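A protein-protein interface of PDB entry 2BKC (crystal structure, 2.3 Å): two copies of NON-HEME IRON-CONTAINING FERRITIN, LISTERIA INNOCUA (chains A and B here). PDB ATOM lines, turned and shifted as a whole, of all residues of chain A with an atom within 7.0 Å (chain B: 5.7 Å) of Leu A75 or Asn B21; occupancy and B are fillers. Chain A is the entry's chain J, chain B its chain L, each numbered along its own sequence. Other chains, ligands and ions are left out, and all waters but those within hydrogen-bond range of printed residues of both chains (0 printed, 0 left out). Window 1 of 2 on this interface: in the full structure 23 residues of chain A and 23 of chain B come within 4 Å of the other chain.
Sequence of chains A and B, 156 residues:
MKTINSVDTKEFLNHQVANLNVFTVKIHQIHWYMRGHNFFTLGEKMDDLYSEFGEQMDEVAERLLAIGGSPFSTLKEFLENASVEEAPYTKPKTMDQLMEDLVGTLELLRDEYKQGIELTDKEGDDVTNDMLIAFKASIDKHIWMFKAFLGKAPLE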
ATOM      1  N   VAL A  22      21.787 -22.460  19.800  1.00  0.00           N
ATOM      2  CA  VAL A  22      22.446 -21.291  19.202  1.00  0.00           C
ATOM      3  C   VAL A  22      23.977 -21.512  19.125  1.00  0.00           C
ATOM      4  O   VAL A  22      24.617 -21.199  18.122  1.00  0.00           O
ATOM      5  CB  VAL A  22      22.111 -19.982  20.011  1.00  0.00           C
ATOM      6  CG1 VAL A  22      22.858 -18.808  19.495  1.00  0.00           C
ATOM      7  CG2 VAL A  22      20.612 -19.672  19.969  1.00  0.00           C
ATOM      8  N   THR A  24      25.647 -24.261  18.916  1.00  0.00           N
ATOM      9  CA  THR A  24      25.925 -25.338  18.005  1.00  0.00           C
ATOM     10  C   THR A  24      25.919 -24.770  16.562  1.00  0.00           C
ATOM     11  O   THR A  24      26.865 -24.957  15.810  1.00  0.00           O
ATOM     12  CB  THR A  24      24.878 -26.444  18.382  1.00  0.00           C
ATOM     13  OG1 THR A  24      25.552 -27.633  18.819  1.00  0.00           O
ATOM     14  CG2 THR A  24      23.890 -26.790  17.345  1.00  0.00           C
ATOM     15  N   VAL A  25      24.927 -23.953  16.246  1.00  0.00           N
ATOM     16  CA  VAL A  25      24.915 -23.205  15.008  1.00  0.00           C
ATOM     17  C   VAL A  25      26.113 -22.231  14.899  1.00  0.00           C
ATOM     18  O   VAL A  25      26.662 -22.056  13.819  1.00  0.00           O
ATOM     19  CB  VAL A  25      23.563 -22.507  14.808  1.00  0.00           C
ATOM     20  CG1 VAL A  25      23.609 -21.515  13.648  1.00  0.00           C
ATOM     21  CG2 VAL A  25      22.467 -23.535  14.567  1.00  0.00           C
ATOM     22  N   HIS A  28      29.325 -24.393  13.927  1.00  0.00           N
ATOM     23  CA  HIS A  28      29.237 -24.545  12.492  1.00  0.00           C
ATOM     24  C   HIS A  28      29.661 -23.265  11.777  1.00  0.00           C
ATOM     25  O   HIS A  28      30.373 -23.320  10.781  1.00  0.00           O
ATOM     26  CB  HIS A  28      27.813 -24.889  12.073  1.00  0.00           C
ATOM     27  CG  HIS A  28      27.542 -26.363  11.924  1.00  0.00           C
ATOM     28  ND1 HIS A  28      28.513 -27.279  11.553  1.00  0.00           N
ATOM     29  CD2 HIS A  28      26.401 -27.077  12.094  1.00  0.00           C
ATOM     30  CE1 HIS A  28      27.975 -28.486  11.480  1.00  0.00           C
ATOM     31  NE2 HIS A  28      26.697 -28.391  11.807  1.00  0.00           N
ATOM     32  N   TRP A  32      32.729 -23.131   9.037  1.00  0.00           N
ATOM     33  CA  TRP A  32      32.508 -22.812   7.637  1.00  0.00           C
ATOM     34  C   TRP A  32      33.324 -21.637   7.152  1.00  0.00           C
ATOM     35  O   TRP A  32      33.692 -21.612   5.995  1.00  0.00           O
ATOM     36  CB  TRP A  32      31.028 -22.583   7.352  1.00  0.00           C
ATOM     37  CG  TRP A  32      30.205 -23.782   7.545  1.00  0.00           C
ATOM     38  CD1 TRP A  32      30.637 -25.090   7.554  1.00  0.00           C
ATOM     39  CD2 TRP A  32      28.798 -23.823   7.795  1.00  0.00           C
ATOM     40  NE1 TRP A  32      29.581 -25.932   7.774  1.00  0.00           N
ATOM     41  CE2 TRP A  32      28.439 -25.189   7.947  1.00  0.00           C
ATOM     42  CE3 TRP A  32      27.803 -22.843   7.973  1.00  0.00           C
ATOM     43  CZ2 TRP A  32      27.119 -25.601   8.226  1.00  0.00           C
ATOM     44  CZ3 TRP A  32      26.489 -23.254   8.232  1.00  0.00           C
ATOM     45  CH2 TRP A  32      26.166 -24.629   8.361  1.00  0.00           C
ATOM     46  N   TYR A  50      31.067 -29.603  17.967  1.00  0.00           N
ATOM     47  CA  TYR A  50      29.711 -29.667  17.465  1.00  0.00           C
ATOM     48  C   TYR A  50      28.964 -30.895  17.977  1.00  0.00           C
ATOM     49  O   TYR A  50      27.882 -30.749  18.515  1.00  0.00           O
ATOM     50  CB  TYR A  50      29.652 -29.627  15.939  1.00  0.00           C
ATOM     51  CG  TYR A  50      28.221 -29.606  15.434  1.00  0.00           C
ATOM     52  CD1 TYR A  50      27.559 -30.776  15.056  1.00  0.00           C
ATOM     53  CD2 TYR A  50      27.520 -28.406  15.351  1.00  0.00           C
ATOM     54  CE1 TYR A  50      26.236 -30.736  14.584  1.00  0.00           C
ATOM     55  CE2 TYR A  50      26.229 -28.353  14.890  1.00  0.00           C
ATOM     56  CZ  TYR A  50      25.589 -29.505  14.525  1.00  0.00           C
ATOM     57  OH  TYR A  50      24.322 -29.399  14.091  1.00  0.00           O
ATOM     58  N   SER A  73      11.295 -26.239  21.393  1.00  0.00           N
ATOM     59  CA  SER A  73      11.514 -27.117  20.259  1.00  0.00           C
ATOM     60  C   SER A  73      11.289 -26.454  18.896  1.00  0.00           C
ATOM     61  O   SER A  73      10.883 -27.126  17.927  1.00  0.00           O
ATOM     62  CB  SER A  73      10.679 -28.386  20.422  1.00  0.00           C
ATOM     63  OG  SER A  73       9.292 -28.166  20.322  1.00  0.00           O
ATOM     64  N   THR A  74      11.609 -25.157  18.831  1.00  0.00           N
ATOM     65  CA  THR A  74      11.624 -24.374  17.601  1.00  0.00           C
ATOM     66  C   THR A  74      12.789 -23.380  17.591  1.00  0.00           C
ATOM     67  O   THR A  74      13.252 -22.952  18.628  1.00  0.00           O
ATOM     68  CB  THR A  74      10.317 -23.549  17.456  1.00  0.00           C
ATOM     69  OG1 THR A  74      10.151 -22.665  18.589  1.00  0.00           O
ATOM     70  CG2 THR A  74       9.087 -24.445  17.422  1.00  0.00           C
ATOM     71  N   LEU A  75      13.230 -23.000  16.404  1.00  0.00           N
ATOM     72  CA  LEU A  75      14.223 -21.940  16.227  1.00  0.00           C
ATOM     73  C   LEU A  75      13.698 -20.621  16.810  1.00  0.00           C
ATOM     74  O   LEU A  75      14.428 -19.910  17.500  1.00  0.00           O
ATOM     75  CB  LEU A  75      14.577 -21.776  14.748  1.00  0.00           C
ATOM     76  CG  LEU A  75      15.528 -22.853  14.191  1.00  0.00           C
ATOM     77  CD1 LEU A  75      14.792 -24.166  13.979  1.00  0.00           C
ATOM     78  CD2 LEU A  75      16.234 -22.401  12.951  1.00  0.00           C
ATOM     79  N   LYS A  76      12.425 -20.324  16.561  1.00  0.00           N
ATOM     80  CA  LYS A  76      11.759 -19.149  17.132  1.00  0.00           C
ATOM     81  C   LYS A  76      11.886 -19.115  18.671  1.00  0.00           C
ATOM     82  O   LYS A  76      12.349 -18.120  19.235  1.00  0.00           O
ATOM     83  CB  LYS A  76      10.284 -19.085  16.644  1.00  0.00           C
ATOM     84  CG  LYS A  76       9.281 -18.308  17.569  1.00  0.00           C
ATOM     85  CD  LYS A  76       8.291 -19.259  18.350  1.00  0.00           C
ATOM     86  CE  LYS A  76       7.856 -18.665  19.736  1.00  0.00           C
ATOM     87  NZ  LYS A  76       6.461 -18.991  20.111  1.00  0.00           N
ATOM     88  N   GLU A  77      11.540 -20.204  19.336  1.00  0.00           N
ATOM     89  CA  GLU A  77      11.660 -20.272  20.794  1.00  0.00           C
ATOM     90  C   GLU A  77      13.093 -20.224  21.309  1.00  0.00           C
ATOM     91  O   GLU A  77      13.324 -19.742  22.411  1.00  0.00           O
ATOM     92  CB  GLU A  77      11.014 -21.534  21.340  1.00  0.00           C
ATOM     93  CG  GLU A  77       9.500 -21.553  21.332  1.00  0.00           C
ATOM     94  CD  GLU A  77       8.976 -22.944  21.681  1.00  0.00           C
ATOM     95  OE1 GLU A  77       9.232 -23.909  20.935  1.00  0.00           O
ATOM     96  OE2 GLU A  77       8.324 -23.094  22.722  1.00  0.00           O
ATOM     97  N   PHE A  78      14.042 -20.766  20.550  1.00  0.00           N
ATOM     98  CA  PHE A  78      15.450 -20.729  20.943  1.00  0.00           C
ATOM     99  C   PHE A  78      15.934 -19.278  20.892  1.00  0.00           C
ATOM    100  O   PHE A  78      16.601 -18.815  21.804  1.00  0.00           O
ATOM    101  CB  PHE A  78      16.361 -21.617  20.050  1.00  0.00           C
ATOM    102  CG  PHE A  78      15.978 -23.085  20.004  1.00  0.00           C
ATOM    103  CD1 PHE A  78      16.251 -23.847  18.874  1.00  0.00           C
ATOM    104  CD2 PHE A  78      15.360 -23.706  21.070  1.00  0.00           C
ATOM    105  CE1 PHE A  78      15.901 -25.196  18.800  1.00  0.00           C
ATOM    106  CE2 PHE A  78      15.025 -25.037  21.002  1.00  0.00           C
ATOM    107  CZ  PHE A  78      15.296 -25.785  19.872  1.00  0.00           C
ATOM    108  N   LEU A  79      15.592 -18.555  19.832  1.00  0.00           N
ATOM    109  CA  LEU A  79      16.001 -17.158  19.718  1.00  0.00           C
ATOM    110  C   LEU A  79      15.359 -16.275  20.811  1.00  0.00           C
ATOM    111  O   LEU A  79      16.006 -15.404  21.368  1.00  0.00           O
ATOM    112  CB  LEU A  79      15.644 -16.608  18.334  1.00  0.00           C
ATOM    113  CG  LEU A  79      16.680 -16.852  17.239  1.00  0.00           C
ATOM    114  CD1 LEU A  79      16.211 -16.213  15.944  1.00  0.00           C
ATOM    115  CD2 LEU A  79      18.012 -16.295  17.653  1.00  0.00           C
ATOM    116  N   GLU A  80      14.107 -16.545  21.136  1.00  0.00           N
ATOM    117  CA  GLU A  80      13.430 -15.791  22.166  1.00  0.00           C
ATOM    118  C   GLU A  80      14.041 -15.961  23.568  1.00  0.00           C
ATOM    119  O   GLU A  80      13.906 -15.058  24.386  1.00  0.00           O
ATOM    120  CB  GLU A  80      11.956 -16.161  22.222  1.00  0.00           C
ATOM    121  CG  GLU A  80      11.105 -15.320  21.293  1.00  0.00           C
ATOM    122  CD  GLU A  80       9.677 -15.859  21.128  1.00  0.00           C
ATOM    123  OE1 GLU A  80       9.324 -16.896  21.780  1.00  0.00           O
ATOM    124  OE2 GLU A  80       8.915 -15.246  20.321  1.00  0.00           O
ATOM    125  N   ASN A  81      14.687 -17.096  23.845  1.00  0.00           N
ATOM    126  CA  ASN A  81      15.143 -17.402  25.211  1.00  0.00           C
ATOM    127  C   ASN A  81      16.653 -17.474  25.440  1.00  0.00           C
ATOM    128  O   ASN A  81      17.106 -17.484  26.586  1.00  0.00           O
ATOM    129  CB  ASN A  81      14.508 -18.703  25.683  1.00  0.00           C
ATOM    130  CG  ASN A  81      12.986 -18.635  25.717  1.00  0.00           C
ATOM    131  OD1 ASN A  81      12.320 -18.875  24.726  1.00  0.00           O
ATOM    132  ND2 ASN A  81      12.439 -18.335  26.869  1.00  0.00           N
ATOM    133  N   GLN B  16      18.188 -24.409   1.098  1.00  0.00           N
ATOM    134  CA  GLN B  16      18.129 -25.703   1.780  1.00  0.00           C
ATOM    135  C   GLN B  16      18.923 -25.777   3.108  1.00  0.00           C
ATOM    136  O   GLN B  16      18.548 -26.531   3.980  1.00  0.00           O
ATOM    137  CB  GLN B  16      18.530 -26.848   0.846  1.00  0.00           C
ATOM    138  CG  GLN B  16      17.645 -27.004  -0.391  1.00  0.00           C
ATOM    139  CD  GLN B  16      16.167 -26.807  -0.093  1.00  0.00           C
ATOM    140  OE1 GLN B  16      15.613 -27.342   0.898  1.00  0.00           O
ATOM    141  NE2 GLN B  16      15.521 -26.051  -0.946  1.00  0.00           N
ATOM    142  N   VAL B  17      19.986 -24.994   3.259  1.00  0.00           N
ATOM    143  CA  VAL B  17      20.687 -24.926   4.530  1.00  0.00           C
ATOM    144  C   VAL B  17      19.702 -24.518   5.606  1.00  0.00           C
ATOM    145  O   VAL B  17      19.699 -25.056   6.709  1.00  0.00           O
ATOM    146  CB  VAL B  17      21.852 -23.905   4.524  1.00  0.00           C
ATOM    147  CG1 VAL B  17      22.499 -23.780   5.919  1.00  0.00           C
ATOM    148  CG2 VAL B  17      22.901 -24.313   3.531  1.00  0.00           C
ATOM    149  N   ALA B  18      18.856 -23.553   5.257  1.00  0.00           N
ATOM    150  CA  ALA B  18      17.817 -23.053   6.135  1.00  0.00           C
ATOM    151  C   ALA B  18      16.782 -24.094   6.427  1.00  0.00           C
ATOM    152  O   ALA B  18      16.474 -24.349   7.582  1.00  0.00           O
ATOM    153  CB  ALA B  18      17.153 -21.837   5.508  1.00  0.00           C
ATOM    154  N   ASN B  19      16.216 -24.677   5.375  1.00  0.00           N
ATOM    155  CA  ASN B  19      15.186 -25.697   5.514  1.00  0.00           C
ATOM    156  C   ASN B  19      15.660 -26.853   6.419  1.00  0.00           C
ATOM    157  O   ASN B  19      14.964 -27.261   7.332  1.00  0.00           O
ATOM    158  CB  ASN B  19      14.803 -26.286   4.151  1.00  0.00           C
ATOM    159  CG  ASN B  19      13.883 -25.372   3.328  1.00  0.00           C
ATOM    160  OD1 ASN B  19      13.220 -24.476   3.853  1.00  0.00           O
ATOM    161  ND2 ASN B  19      13.824 -25.633   2.022  1.00  0.00           N
ATOM    162  N   LEU B  20      16.871 -27.327   6.180  1.00  0.00           N
ATOM    163  CA  LEU B  20      17.391 -28.500   6.876  1.00  0.00           C
ATOM    164  C   LEU B  20      17.714 -28.175   8.353  1.00  0.00           C
ATOM    165  O   LEU B  20      17.529 -29.058   9.201  1.00  0.00           O
ATOM    166  CB  LEU B  20      18.632 -29.037   6.173  1.00  0.00           C
ATOM    167  CG  LEU B  20      18.624 -30.213   5.175  1.00  0.00           C
ATOM    168  CD1 LEU B  20      17.296 -30.737   4.695  1.00  0.00           C
ATOM    169  CD2 LEU B  20      19.491 -29.835   3.968  1.00  0.00           C
ATOM    170  N   ASN B  21      18.192 -26.955   8.658  1.00  0.00           N
ATOM    171  CA  ASN B  21      18.353 -26.546  10.064  1.00  0.00           C
ATOM    172  C   ASN B  21      17.007 -26.392  10.771  1.00  0.00           C
ATOM    173  O   ASN B  21      16.943 -26.540  11.984  1.00  0.00           O
ATOM    174  CB  ASN B  21      19.192 -25.284  10.228  1.00  0.00           C
ATOM    175  CG  ASN B  21      20.690 -25.591  10.317  1.00  0.00           C
ATOM    176  OD1 ASN B  21      21.160 -26.080  11.343  1.00  0.00           O
ATOM    177  ND2 ASN B  21      21.430 -25.371   9.215  1.00  0.00           N
ATOM    178  N   VAL B  22      15.931 -26.136  10.027  1.00  0.00           N
ATOM    179  CA  VAL B  22      14.586 -26.101  10.628  1.00  0.00           C
ATOM    180  C   VAL B  22      14.078 -27.540  10.820  1.00  0.00           C
ATOM    181  O   VAL B  22      13.587 -27.872  11.892  1.00  0.00           O
ATOM    182  CB  VAL B  22      13.591 -25.255   9.789  1.00  0.00           C
ATOM    183  CG1 VAL B  22      12.179 -25.383  10.341  1.00  0.00           C
ATOM    184  CG2 VAL B  22      13.979 -23.795   9.784  1.00  0.00           C
ATOM    185  N   PHE B  23      14.220 -28.393   9.788  1.00  0.00           N
ATOM    186  CA  PHE B  23      13.744 -29.779   9.816  1.00  0.00           C
ATOM    187  C   PHE B  23      14.429 -30.578  10.939  1.00  0.00           C
ATOM    188  O   PHE B  23      13.815 -31.374  11.670  1.00  0.00           O
ATOM    189  CB  PHE B  23      13.999 -30.379   8.434  1.00  0.00           C
ATOM    190  CG  PHE B  23      13.488 -31.759   8.237  1.00  0.00           C
ATOM    191  CD1 PHE B  23      12.192 -32.081   8.485  1.00  0.00           C
ATOM    192  CD2 PHE B  23      14.313 -32.744   7.717  1.00  0.00           C
ATOM    193  CE1 PHE B  23      11.718 -33.376   8.262  1.00  0.00           C
ATOM    194  CE2 PHE B  23      13.828 -34.039   7.484  1.00  0.00           C
ATOM    195  CZ  PHE B  23      12.544 -34.346   7.783  1.00  0.00           C
ATOM    196  N   THR B  24      15.697 -30.288  11.101  1.00  0.00           N
ATOM    197  CA  THR B  24      16.555 -30.949  12.078  1.00  0.00           C
ATOM    198  C   THR B  24      15.963 -30.762  13.509  1.00  0.00           C
ATOM    199  O   THR B  24      15.725 -31.740  14.221  1.00  0.00           O
ATOM    200  CB  THR B  24      18.030 -30.433  11.826  1.00  0.00           C
ATOM    201  OG1 THR B  24      18.864 -31.519  11.358  1.00  0.00           O
ATOM    202  CG2 THR B  24      18.727 -29.860  13.004  1.00  0.00           C
ATOM    203  N   VAL B  25      15.636 -29.516  13.847  1.00  0.00           N
ATOM    204  CA  VAL B  25      14.997 -29.135  15.112  1.00  0.00           C
ATOM    205  C   VAL B  25      13.591 -29.752  15.228  1.00  0.00           C
ATOM    206  O   VAL B  25      13.219 -30.302  16.278  1.00  0.00           O
ATOM    207  CB  VAL B  25      15.045 -27.582  15.303  1.00  0.00           C
ATOM    208  CG1 VAL B  25      14.154 -27.116  16.486  1.00  0.00           C
ATOM    209  CG2 VAL B  25      16.529 -27.129  15.503  1.00  0.00           C
ATOM    210  N   LYS B  26      12.858 -29.762  14.127  1.00  0.00           N
ATOM    211  CA  LYS B  26      11.564 -30.443  14.094  1.00  0.00           C
ATOM    212  C   LYS B  26      11.681 -31.950  14.421  1.00  0.00           C
ATOM    213  O   LYS B  26      10.821 -32.500  15.097  1.00  0.00           O
ATOM    214  CB  LYS B  26      10.895 -30.210  12.758  1.00  0.00           C
ATOM    215  CG  LYS B  26       9.414 -30.648  12.634  1.00  0.00           C
ATOM    216  CD  LYS B  26       8.970 -30.665  11.137  1.00  0.00           C
ATOM    217  CE  LYS B  26       8.140 -29.436  10.720  1.00  0.00           C
ATOM    218  NZ  LYS B  26       6.942 -29.222  11.634  1.00  0.00           N
ATOM    219  N   MET B  57      22.813 -31.476   5.521  1.00  0.00           N
ATOM    220  CA  MET B  57      22.916 -30.052   5.741  1.00  0.00           C
ATOM    221  C   MET B  57      24.356 -29.654   5.636  1.00  0.00           C
ATOM    222  O   MET B  57      24.690 -28.740   4.961  1.00  0.00           O
ATOM    223  CB  MET B  57      22.346 -29.713   7.112  1.00  0.00           C
ATOM    224  CG  MET B  57      22.132 -28.234   7.351  1.00  0.00           C
ATOM    225  SD  MET B  57      23.585 -27.436   7.893  1.00  0.00           S
ATOM    226  CE  MET B  57      23.783 -28.157   9.639  1.00  0.00           C
ATOM    227  N   LEU B  75      20.522 -18.853  13.534  1.00  0.00           N
ATOM    228  CA  LEU B  75      19.105 -19.223  13.584  1.00  0.00           C
ATOM    229  C   LEU B  75      18.244 -18.162  12.902  1.00  0.00           C
ATOM    230  O   LEU B  75      17.255 -18.468  12.245  1.00  0.00           O
ATOM    231  CB  LEU B  75      18.624 -19.422  15.034  1.00  0.00           C
ATOM    232  CG  LEU B  75      18.829 -20.802  15.649  1.00  0.00           C
ATOM    233  CD1 LEU B  75      20.294 -21.074  15.790  1.00  0.00           C
ATOM    234  CD2 LEU B  75      18.162 -20.872  17.022  1.00  0.00           C
ATOM    235  N   PHE B  78      18.234 -18.610   9.227  1.00  0.00           N
ATOM    236  CA  PHE B  78      17.474 -19.811   8.825  1.00  0.00           C
ATOM    237  C   PHE B  78      16.004 -19.525   8.838  1.00  0.00           C
ATOM    238  O   PHE B  78      15.305 -19.900   7.904  1.00  0.00           O
ATOM    239  CB  PHE B  78      17.749 -21.077   9.684  1.00  0.00           C
ATOM    240  CG  PHE B  78      19.205 -21.425   9.822  1.00  0.00           C
ATOM    241  CD1 PHE B  78      19.654 -22.074  10.952  1.00  0.00           C
ATOM    242  CD2 PHE B  78      20.131 -21.071   8.838  1.00  0.00           C
ATOM    243  CE1 PHE B  78      20.998 -22.381  11.097  1.00  0.00           C
ATOM    244  CE2 PHE B  78      21.469 -21.374   8.997  1.00  0.00           C
ATOM    245  CZ  PHE B  78      21.899 -22.027  10.117  1.00  0.00           C
ATOM    246  N   LEU B  79      15.535 -18.854   9.885  1.00  0.00           N
ATOM    247  CA  LEU B  79      14.122 -18.471   9.971  1.00  0.00           C
ATOM    248  C   LEU B  79      13.739 -17.534   8.841  1.00  0.00           C
ATOM    249  O   LEU B  79      12.672 -17.672   8.277  1.00  0.00           O
ATOM    250  CB  LEU B  79      13.799 -17.843  11.323  1.00  0.00           C
ATOM    251  CG  LEU B  79      13.511 -18.813  12.472  1.00  0.00           C
ATOM    252  CD1 LEU B  79      13.147 -18.012  13.701  1.00  0.00           C
ATOM    253  CD2 LEU B  79      12.395 -19.831  12.135  1.00  0.00           C
ATOM    254  N   GLU B  86       7.531 -24.467  11.203  1.00  0.00           N
ATOM    255  CA  GLU B  86       7.528 -25.035  12.534  1.00  0.00           C
ATOM    256  C   GLU B  86       6.450 -24.361  13.355  1.00  0.00           C
ATOM    257  O   GLU B  86       6.010 -23.263  13.038  1.00  0.00           O
ATOM    258  CB  GLU B  86       8.867 -24.809  13.218  1.00  0.00           C
ATOM    259  CG  GLU B  86       9.383 -23.368  13.132  1.00  0.00           C
ATOM    260  CD  GLU B  86      10.662 -23.140  13.919  1.00  0.00           C
ATOM    261  OE1 GLU B  86      10.783 -22.012  14.459  1.00  0.00           O
ATOM    262  OE2 GLU B  86      11.532 -24.065  13.998  1.00  0.00           O
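The backbone NH (N) of Leu A75 is in hydrogen-bond range of the side-chain carboxylate (OE2) of Glu B86 (3.1 Å).
The side-chain carboxylate (OE1) of Glu B86 lies within hydrogen-bond range of the backbone NH (N) of Lys A76 (3.2 Å).
The side-chain amino group (NZ) of Lys A76 lies within salt-bridge range of the side-chain carboxylate (OE1) of Glu A80 (3.9 Å).
The side-chain carboxylate (OE1) of Glu A77 is in hydrogen-bond range of the side-chain hydroxyl (OG1) of Thr A74 (2.8 Å).
The backbone carbonyl oxygen of Val B17 sits at hydrogen-bond distance from the side-chain amide nitrogen of Asn B21.
The side-chain amide nitrogen (ND2) of Asn B21 sits at hydrogen-bond distance from the side-chain sulfur (SD) of Met B57 (3.3 Å).
The backbone NH (N) of Ser A73 lies within hydrogen-bond range of the side-chain carboxylate (OE1) of Glu A77 (3.1 Å).
A ring nitrogen (NE2) of His A28 sits close to the side-chain hydroxyl (OH) of Tyr A50.
Among the printed residues, pairs that only touch across the chains: Thr A74 with Glu B86, Phe A78 with Val B25, Val A25 with Leu B75, Ser A73 with Val B25, Phe A78 with Leu B75, His A28 with Met B57, Leu A75 with Val B25, Lys A76 with Leu B79, Val A25 with Phe B78, Leu A75 with Asn B21, Leu A75 with Phe B78, Trp A32 with Met B57, Leu A75 with Val B22, Leu A75 with Leu B79, Leu A75 with Leu B75, Thr A74 with Val B25 and Leu A79 with Leu B75.
Leu A75 touches seven residues of chain B.
Asn B21 touches just one residue of chain A: Leu A75.
Printed residues of chain B within 4 Å of Leu A79: Leu B75 (3.9 Å).
Printed residues of chain B within 4 Å of Val A25: Leu B75 and Phe B78.
Of the printed residues of chain A, Val B22 touches Leu A75 (3.9 Å).
Of the printed residues of chain B, Thr A74 touches Val B25 and Glu B86.
The nearest printed residue of chain B that does not touch Leu A75 is Ala B18 (5.7 Å).
The nearest residue of chain A that does not touch Asn B21 is Val A25 (4.3 Å).
The nearest printed residue of chain A that does not touch Glu B86 is Ser A73 (5.0 Å).
Of the 15 printed residues of chain A, 9 touch a printed residue of chain B.
Printed residues of chain A that touch a printed residue of chain B: Val A25, His A28, Trp A32, Ser A73, Thr A74, Leu A75, Lys A76, Phe A78 and Leu A79.
Hydrophobic or aromatic side chains of chain A that line the printed part of chain B: Val A25, His A28, Trp A32, Leu A75, Phe A78 and Leu A79.
Among the printed residues, 19 pairs touch across the chains.
Val A25 touches Phe B78, and with the chains exchanged Phe A78 touches Val B25.
Leu B75 touches its own counterpart, Leu A75.
Leu A75 touches Phe B78, and with the chains exchanged Phe A78 touches Leu B75.
Leu A75 touches Leu B79, and with the chains exchanged Leu A79 touches Leu B75.
Positions printed for both chains: 22, 24, 25, 75, 78 and 79.
Of the 19 pairs that touch across the chains among the printed residues, 9 have their exchanged pair printed and touching as well.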
